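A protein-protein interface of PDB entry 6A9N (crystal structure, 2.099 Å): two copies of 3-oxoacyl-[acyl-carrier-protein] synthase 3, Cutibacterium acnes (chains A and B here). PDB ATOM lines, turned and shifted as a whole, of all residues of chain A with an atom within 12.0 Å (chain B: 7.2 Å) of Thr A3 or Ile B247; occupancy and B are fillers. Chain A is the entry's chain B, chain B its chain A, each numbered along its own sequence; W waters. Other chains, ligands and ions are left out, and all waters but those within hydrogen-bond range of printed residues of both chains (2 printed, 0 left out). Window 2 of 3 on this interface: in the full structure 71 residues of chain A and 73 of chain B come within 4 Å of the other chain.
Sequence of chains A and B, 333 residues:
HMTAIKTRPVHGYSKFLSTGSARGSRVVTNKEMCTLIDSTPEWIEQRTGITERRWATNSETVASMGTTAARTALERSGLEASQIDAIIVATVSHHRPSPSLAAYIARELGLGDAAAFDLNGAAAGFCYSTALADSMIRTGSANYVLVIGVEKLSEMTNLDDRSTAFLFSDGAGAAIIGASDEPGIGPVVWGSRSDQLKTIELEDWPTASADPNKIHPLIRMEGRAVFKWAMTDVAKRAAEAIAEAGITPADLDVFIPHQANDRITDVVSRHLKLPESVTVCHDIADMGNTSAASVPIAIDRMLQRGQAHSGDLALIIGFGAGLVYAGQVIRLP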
ATOM      1  N   THR A   3      14.192  27.310 -18.779  1.00  0.00           N
ATOM      2  CA  THR A   3      14.340  26.042 -19.516  1.00  0.00           C
ATOM      3  C   THR A   3      13.092  25.146 -19.476  1.00  0.00           C
ATOM      4  O   THR A   3      12.585  24.808 -18.407  1.00  0.00           O
ATOM      5  CB  THR A   3      15.542  25.238 -18.990  1.00  0.00           C
ATOM      6  OG1 THR A   3      16.688  26.086 -18.959  1.00  0.00           O
ATOM      7  CG2 THR A   3      15.848  24.022 -19.896  1.00  0.00           C
ATOM      8  N   ALA A   4      12.611  24.753 -20.656  1.00  0.00           N
ATOM      9  CA  ALA A   4      11.410  23.943 -20.796  1.00  0.00           C
ATOM     10  C   ALA A   4      11.729  22.454 -20.680  1.00  0.00           C
ATOM     11  O   ALA A   4      12.867  22.019 -20.858  1.00  0.00           O
ATOM     12  CB  ALA A   4      10.731  24.214 -22.140  1.00  0.00           C
ATOM     13  N   ILE A   5      10.697  21.673 -20.366  1.00  0.00           N
ATOM     14  CA  ILE A   5      10.753  20.225 -20.495  1.00  0.00           C
ATOM     15  C   ILE A   5       9.652  19.810 -21.458  1.00  0.00           C
ATOM     16  O   ILE A   5       8.723  20.575 -21.737  1.00  0.00           O
ATOM     17  CB  ILE A   5      10.609  19.487 -19.140  1.00  0.00           C
ATOM     18  CG1 ILE A   5       9.333  19.921 -18.408  1.00  0.00           C
ATOM     19  CG2 ILE A   5      11.859  19.688 -18.285  1.00  0.00           C
ATOM     20  CD1 ILE A   5       9.339  19.592 -16.914  1.00  0.00           C
ATOM     21  N   LYS A   6       9.772  18.598 -21.990  1.00  0.00           N
ATOM     22  CA  LYS A   6       8.756  18.085 -22.899  1.00  0.00           C
ATOM     23  C   LYS A   6       8.053  16.873 -22.291  1.00  0.00           C
ATOM     24  O   LYS A   6       8.414  16.382 -21.215  1.00  0.00           O
ATOM     25  CB  LYS A   6       9.360  17.736 -24.267  1.00  0.00           C
ATOM     26  CG  LYS A   6      10.437  16.680 -24.257  1.00  0.00           C
ATOM     27  CD  LYS A   6      10.911  16.333 -25.680  1.00  0.00           C
ATOM     28  CE  LYS A   6      11.858  15.128 -25.640  1.00  0.00           C
ATOM     29  NZ  LYS A   6      12.475  14.813 -26.961  1.00  0.00           N
ATOM     30  N   THR A   7       7.031  16.405 -23.008  1.00  0.00           N
ATOM     31  CA  THR A   7       6.243  15.231 -22.648  1.00  0.00           C
ATOM     32  C   THR A   7       6.135  14.315 -23.867  1.00  0.00           C
ATOM     33  O   THR A   7       6.371  14.740 -24.997  1.00  0.00           O
ATOM     34  CB  THR A   7       4.840  15.628 -22.149  1.00  0.00           C
ATOM     35  OG1 THR A   7       4.130  16.324 -23.181  1.00  0.00           O
ATOM     36  CG2 THR A   7       4.936  16.541 -20.926  1.00  0.00           C
ATOM     37  N   ARG A   8       5.783  13.045 -23.633  1.00  0.00           N
ATOM     38  CA  ARG A   8       5.715  12.071 -24.717  1.00  0.00           C
ATOM     39  C   ARG A   8       4.601  12.405 -25.712  1.00  0.00           C
ATOM     40  O   ARG A   8       3.540  12.917 -25.329  1.00  0.00           O
ATOM     41  CB  ARG A   8       5.488  10.665 -24.169  1.00  0.00           C
ATOM     42  CG  ARG A   8       6.766   9.974 -23.779  1.00  0.00           C
ATOM     43  CD  ARG A   8       6.514   8.556 -23.298  1.00  0.00           C
ATOM     44  NE  ARG A   8       7.720   8.009 -22.695  1.00  0.00           N
ATOM     45  CZ  ARG A   8       7.874   7.762 -21.396  1.00  0.00           C
ATOM     46  NH1 ARG A   8       6.883   8.001 -20.540  1.00  0.00           N
ATOM     47  NH2 ARG A   8       9.023   7.262 -20.955  1.00  0.00           N
ATOM     48  N   PRO B 183       4.325  22.021 -19.722  1.00  0.00           N
ATOM     49  CA  PRO B 183       4.719  20.796 -18.997  1.00  0.00           C
ATOM     50  C   PRO B 183       5.445  21.106 -17.693  1.00  0.00           C
ATOM     51  O   PRO B 183       6.493  21.751 -17.685  1.00  0.00           O
ATOM     52  CB  PRO B 183       5.638  20.077 -19.993  1.00  0.00           C
ATOM     53  CG  PRO B 183       5.304  20.663 -21.316  1.00  0.00           C
ATOM     54  CD  PRO B 183       4.886  22.073 -21.080  1.00  0.00           C
ATOM     55  N   ALA B 239      19.363   8.643 -16.190  1.00  0.00           N
ATOM     56  CA  ALA B 239      19.826   9.350 -17.383  1.00  0.00           C
ATOM     57  C   ALA B 239      18.745   9.390 -18.453  1.00  0.00           C
ATOM     58  O   ALA B 239      18.559  10.420 -19.110  1.00  0.00           O
ATOM     59  CB  ALA B 239      21.097   8.696 -17.933  1.00  0.00           C
ATOM     60  N   ALA B 241      15.500   9.312 -17.840  1.00  0.00           N
ATOM     61  CA  ALA B 241      14.447  10.232 -17.426  1.00  0.00           C
ATOM     62  C   ALA B 241      14.808  11.670 -17.789  1.00  0.00           C
ATOM     63  O   ALA B 241      13.938  12.459 -18.164  1.00  0.00           O
ATOM     64  CB  ALA B 241      14.179  10.097 -15.925  1.00  0.00           C
ATOM     65  N   ILE B 242      16.084  12.030 -17.662  1.00  0.00           N
ATOM     66  CA  ILE B 242      16.521  13.371 -18.038  1.00  0.00           C
ATOM     67  C   ILE B 242      16.312  13.588 -19.534  1.00  0.00           C
ATOM     68  O   ILE B 242      15.724  14.589 -19.966  1.00  0.00           O
ATOM     69  CB  ILE B 242      17.990  13.579 -17.627  1.00  0.00           C
ATOM     70  CG1 ILE B 242      18.117  13.531 -16.097  1.00  0.00           C
ATOM     71  CG2 ILE B 242      18.523  14.912 -18.140  1.00  0.00           C
ATOM     72  CD1 ILE B 242      19.550  13.536 -15.612  1.00  0.00           C
ATOM     73  N   ALA B 243      16.753  12.620 -20.341  1.00  0.00           N
ATOM     74  CA  ALA B 243      16.651  12.724 -21.794  1.00  0.00           C
ATOM     75  C   ALA B 243      15.200  12.805 -22.247  1.00  0.00           C
ATOM     76  O   ALA B 243      14.853  13.652 -23.073  1.00  0.00           O
ATOM     77  CB  ALA B 243      17.360  11.541 -22.451  1.00  0.00           C
ATOM     78  N   GLU B 244      14.323  11.952 -21.691  1.00  0.00           N
ATOM     79  CA  GLU B 244      12.908  11.981 -22.083  1.00  0.00           C
ATOM     80  C   GLU B 244      12.270  13.337 -21.820  1.00  0.00           C
ATOM     81  O   GLU B 244      11.290  13.709 -22.484  1.00  0.00           O
ATOM     82  CB  GLU B 244      12.118  10.905 -21.335  1.00  0.00           C
ATOM     83  CG  GLU B 244      12.464   9.486 -21.749  1.00  0.00           C
ATOM     84  CD  GLU B 244      11.977   9.161 -23.161  1.00  0.00           C
ATOM     85  OE1 GLU B 244      10.910   9.670 -23.556  1.00  0.00           O
ATOM     86  OE2 GLU B 244      12.660   8.403 -23.874  1.00  0.00           O
ATOM     87  N   ALA B 245      12.783  14.071 -20.834  1.00  0.00           N
ATOM     88  CA  ALA B 245      12.292  15.403 -20.536  1.00  0.00           C
ATOM     89  C   ALA B 245      12.841  16.457 -21.496  1.00  0.00           C
ATOM     90  O   ALA B 245      12.413  17.615 -21.428  1.00  0.00           O
ATOM     91  CB  ALA B 245      12.632  15.770 -19.082  1.00  0.00           C
ATOM     92  N   GLY B 246      13.754  16.081 -22.389  1.00  0.00           N
ATOM     93  CA  GLY B 246      14.268  17.010 -23.379  1.00  0.00           C
ATOM     94  C   GLY B 246      15.270  18.007 -22.843  1.00  0.00           C
ATOM     95  O   GLY B 246      15.319  19.145 -23.324  1.00  0.00           O
ATOM     96  N   ILE B 247      16.059  17.611 -21.843  1.00  0.00           N
ATOM     97  CA  ILE B 247      17.092  18.441 -21.245  1.00  0.00           C
ATOM     98  C   ILE B 247      18.328  17.571 -21.057  1.00  0.00           C
ATOM     99  O   ILE B 247      18.287  16.344 -21.200  1.00  0.00           O
ATOM    100  CB  ILE B 247      16.667  19.065 -19.890  1.00  0.00           C
ATOM    101  CG1 ILE B 247      16.114  17.997 -18.943  1.00  0.00           C
ATOM    102  CG2 ILE B 247      15.641  20.181 -20.072  1.00  0.00           C
ATOM    103  CD1 ILE B 247      16.261  18.386 -17.461  1.00  0.00           C
ATOM    104  N   THR B 248      19.431  18.229 -20.744  1.00  0.00           N
ATOM    105  CA  THR B 248      20.682  17.616 -20.357  1.00  0.00           C
ATOM    106  C   THR B 248      20.827  17.671 -18.846  1.00  0.00           C
ATOM    107  O   THR B 248      20.106  18.416 -18.177  1.00  0.00           O
ATOM    108  CB  THR B 248      21.865  18.353 -21.000  1.00  0.00           C
ATOM    109  OG1 THR B 248      22.004  19.633 -20.374  1.00  0.00           O
ATOM    110  CG2 THR B 248      21.654  18.530 -22.517  1.00  0.00           C
ATOM    111  N   PRO B 249      21.755  16.893 -18.274  1.00  0.00           N
ATOM    112  CA  PRO B 249      22.000  16.999 -16.822  1.00  0.00           C
ATOM    113  C   PRO B 249      22.317  18.405 -16.344  1.00  0.00           C
ATOM    114  O   PRO B 249      21.831  18.812 -15.281  1.00  0.00           O
ATOM    115  CB  PRO B 249      23.182  16.046 -16.609  1.00  0.00           C
ATOM    116  CG  PRO B 249      22.932  14.954 -17.634  1.00  0.00           C
ATOM    117  CD  PRO B 249      22.390  15.689 -18.855  1.00  0.00           C
ATOM    118  N   ALA B 250      23.101  19.171 -17.108  1.00  0.00           N
ATOM    119  CA  ALA B 250      23.464  20.518 -16.692  1.00  0.00           C
ATOM    120  C   ALA B 250      22.277  21.469 -16.655  1.00  0.00           C
ATOM    121  O   ALA B 250      22.369  22.523 -16.017  1.00  0.00           O
ATOM    122  CB  ALA B 250      24.544  21.073 -17.618  1.00  0.00           C
ATOM    123  N   ASP B 251      21.167  21.134 -17.321  1.00  0.00           N
ATOM    124  CA  ASP B 251      19.962  21.949 -17.218  1.00  0.00           C
ATOM    125  C   ASP B 251      19.217  21.734 -15.907  1.00  0.00           C
ATOM    126  O   ASP B 251      18.371  22.563 -15.549  1.00  0.00           O
ATOM    127  CB  ASP B 251      19.003  21.645 -18.375  1.00  0.00           C
ATOM    128  CG  ASP B 251      19.571  22.039 -19.722  1.00  0.00           C
ATOM    129  OD1 ASP B 251      20.106  23.168 -19.843  1.00  0.00           O
ATOM    130  OD2 ASP B 251      19.486  21.210 -20.655  1.00  0.00           O
ATOM    131  N   LEU B 252      19.485  20.631 -15.210  1.00  0.00           N
ATOM    132  CA  LEU B 252      18.865  20.401 -13.914  1.00  0.00           C
ATOM    133  C   LEU B 252      19.328  21.448 -12.913  1.00  0.00           C
ATOM    134  O   LEU B 252      20.477  21.892 -12.934  1.00  0.00           O
ATOM    135  CB  LEU B 252      19.218  19.015 -13.387  1.00  0.00           C
ATOM    136  CG  LEU B 252      18.555  17.819 -14.058  1.00  0.00           C
ATOM    137  CD1 LEU B 252      19.055  16.573 -13.401  1.00  0.00           C
ATOM    138  CD2 LEU B 252      17.027  17.922 -13.961  1.00  0.00           C
ATOM    139  N   ASP B 253      18.426  21.842 -12.023  1.00  0.00           N
ATOM    140  CA  ASP B 253      18.845  22.609 -10.864  1.00  0.00           C
ATOM    141  C   ASP B 253      19.070  21.748  -9.636  1.00  0.00           C
ATOM    142  O   ASP B 253      19.870  22.117  -8.767  1.00  0.00           O
ATOM    143  CB  ASP B 253      17.809  23.683 -10.573  1.00  0.00           C
ATOM    144  CG  ASP B 253      17.582  24.587 -11.772  1.00  0.00           C
ATOM    145  OD1 ASP B 253      18.510  25.355 -12.097  1.00  0.00           O
ATOM    146  OD2 ASP B 253      16.499  24.509 -12.403  1.00  0.00           O
ATOM    147  N   GLY B 311      10.411  26.974  -9.522  1.00  0.00           N
ATOM    148  CA  GLY B 311      10.843  27.084 -10.895  1.00  0.00           C
ATOM    149  C   GLY B 311      12.039  26.235 -11.254  1.00  0.00           C
ATOM    150  O   GLY B 311      12.325  26.084 -12.447  1.00  0.00           O
ATOM    151  N   LEU B 313      14.214  22.961 -12.070  1.00  0.00           N
ATOM    152  CA  LEU B 313      14.008  21.620 -12.596  1.00  0.00           C
ATOM    153  C   LEU B 313      14.713  20.622 -11.685  1.00  0.00           C
ATOM    154  O   LEU B 313      15.897  20.785 -11.377  1.00  0.00           O
ATOM    155  CB  LEU B 313      14.540  21.503 -14.022  1.00  0.00           C
ATOM    156  CG  LEU B 313      13.793  22.307 -15.078  1.00  0.00           C
ATOM    157  CD1 LEU B 313      14.423  22.024 -16.439  1.00  0.00           C
ATOM    158  CD2 LEU B 313      12.292  21.984 -15.057  1.00  0.00           C
ATOM    159  N   ALA B 314      13.978  19.598 -11.255  1.00  0.00           N
ATOM    160  CA  ALA B 314      14.487  18.567 -10.356  1.00  0.00           C
ATOM    161  C   ALA B 314      14.247  17.209 -10.987  1.00  0.00           C
ATOM    162  O   ALA B 314      13.131  16.920 -11.423  1.00  0.00           O
ATOM    163  CB  ALA B 314      13.790  18.610  -8.987  1.00  0.00           C
ATOM    164  N   LEU B 315      15.291  16.387 -11.042  1.00  0.00           N
ATOM    165  CA  LEU B 315      15.113  14.971 -11.303  1.00  0.00           C
ATOM    166  C   LEU B 315      14.796  14.275  -9.984  1.00  0.00           C
ATOM    167  O   LEU B 315      15.599  14.333  -9.044  1.00  0.00           O
ATOM    168  CB  LEU B 315      16.369  14.380 -11.933  1.00  0.00           C
ATOM    169  CG  LEU B 315      16.344  12.858 -12.002  1.00  0.00           C
ATOM    170  CD1 LEU B 315      15.312  12.379 -13.037  1.00  0.00           C
ATOM    171  CD2 LEU B 315      17.729  12.345 -12.327  1.00  0.00           C
ATOM    172  N   VAL B 329      11.584  14.143 -14.444  1.00  0.00           N
ATOM    173  CA  VAL B 329      11.951  15.528 -14.175  1.00  0.00           C
ATOM    174  C   VAL B 329      10.679  16.317 -13.910  1.00  0.00           C
ATOM    175  O   VAL B 329       9.686  16.176 -14.635  1.00  0.00           O
ATOM    176  CB  VAL B 329      12.751  16.133 -15.344  1.00  0.00           C
ATOM    177  CG1 VAL B 329      13.086  17.615 -15.050  1.00  0.00           C
ATOM    178  CG2 VAL B 329      14.024  15.325 -15.587  1.00  0.00           C
ATOM    179  N   ARG B 331       9.125  20.342 -12.365  1.00  0.00           N
ATOM    180  CA  ARG B 331       9.376  21.725 -11.990  1.00  0.00           C
ATOM    181  C   ARG B 331       8.856  21.958 -10.579  1.00  0.00           C
ATOM    182  O   ARG B 331       7.682  21.697 -10.300  1.00  0.00           O
ATOM    183  CB  ARG B 331       8.718  22.714 -12.956  1.00  0.00           C
ATOM    184  CG  ARG B 331       9.273  24.148 -12.749  1.00  0.00           C
ATOM    185  CD  ARG B 331       8.839  25.142 -13.803  1.00  0.00           C
ATOM    186  NE  ARG B 331       9.077  24.658 -15.166  1.00  0.00           N
ATOM    187  CZ  ARG B 331      10.234  24.747 -15.817  1.00  0.00           C
ATOM    188  NH1 ARG B 331      11.298  25.313 -15.248  1.00  0.00           N
ATOM    189  NH2 ARG B 331      10.322  24.273 -17.055  1.00  0.00           N
HETATM  190  O   HOH W   1       8.367  23.180 -19.012  1.00  0.00           O
HETATM  191  O   HOH W   2      14.211  26.079 -15.571  1.00  0.00           O
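Water W1 lies within hydrogen-bond range of the backbone carbonyl oxygen (O) of Pro B183 (2.7 Å), the guanidinium group (NH2) of Arg B331 (3.0 Å) and the backbone NH (N) of Ile A5 (3.1 Å). Water W2 lies within hydrogen-bond range of the guanidinium group of Arg B331 and the backbone NH of Thr A3.
The backbone NH (N) of Lys A6 is in hydrogen-bond range of the backbone carbonyl oxygen (O) of Ala B245, 2.9 Å away. The backbone carbonyl oxygen (O) of Thr A3 is in hydrogen-bond range of the guanidinium group (NH2) of Arg B331 (2.7 Å). The guanidinium group (NE) of Arg A8 lies within salt-bridge range of the side-chain carboxylate (OE1) of Glu B244 (3.7 Å).
No position is printed for both chains.
Ile B247 touches Thr A3. Thr A3 touches Leu B313. Ile B247 touches Ala A4. Arg B331 touches Ala A4 (NH2 to CA, 3.9 Å). Ile A5 touches Pro B183 (O to CG, 3.4 Å). Ala B245 touches Ile A5. Ile A5 touches Leu B313 (CG2 to CD1, 3.9 Å). Glu B244 touches Lys A6 (O to CE, 3.5 Å). CA of Gly B246 touches CE of Lys A6, 3.8 Å away. Thr A7 touches Pro B183 (CG2 to CB, 3.7 Å).
Thr A3 touches three residues of chain B. Of chain A, only Thr A3 and Ala A4 come within 4 Å of Ile B247. No residue of chain A comes within 4 Å of Ile B242. No residue of chain A comes within 4 Å of Ala B243. Ala B245 touches two residues of chain A. Of chain A, only Lys A6 (3.8 Å) comes within 4 Å of Gly B246. No residue of chain A comes within 4 Å of Thr B248. Pro B249 touches none of the printed residues of chain A. No residue of chain A comes within 4 Å of Asp B251. No residue of chain A comes within 4 Å of Leu B252. Of the printed residues of chain B, Thr A7 touches Pro B183. Printed residues of chain A within 4 Å of Arg B331: Thr A3 and Ala A4. Of the printed residues of chain B, Ala A4 touches Ile B247 (3.4 Å) and Arg B331 (3.9 Å). Of the printed residues of chain A, Pro B183 touches Ile A5 and Thr A7. Of the printed residues of chain B, Arg A8 touches Glu B244. Ala B239 touches none of the printed residues of chain A. Asp B253 touches none of the printed residues of chain A. The nearest residue of chain B that does not touch Thr A3 is Asp B251 (4.2 Å). The nearest residue of chain A that does not touch Ile B247 is Ile A5 (4.2 Å).
Hydrophobic or aromatic side chains of chain A that line the printed part of chain B: Ile A5. Of the 21 printed residues of chain B, 7 touch a printed residue of chain A. Hydrophobic or aromatic side chains of chain B within 4 Å of the printed part of chain A: Pro B183, Ile B247 and Leu B313. Among the printed residues, Asp or Glu carboxylates within 4 Å of a Lys or Arg side-chain nitrogen of the other chain: Arg A8 with Glu B244 (3.7 Å).
N of Leu B313 sits at hydrogen-bond distance from OD2 of Asp B253, at 2.8 Å. The backbone carbonyl oxygen of Gly B311 lies within hydrogen-bond range of the guanidinium group of Arg B331.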
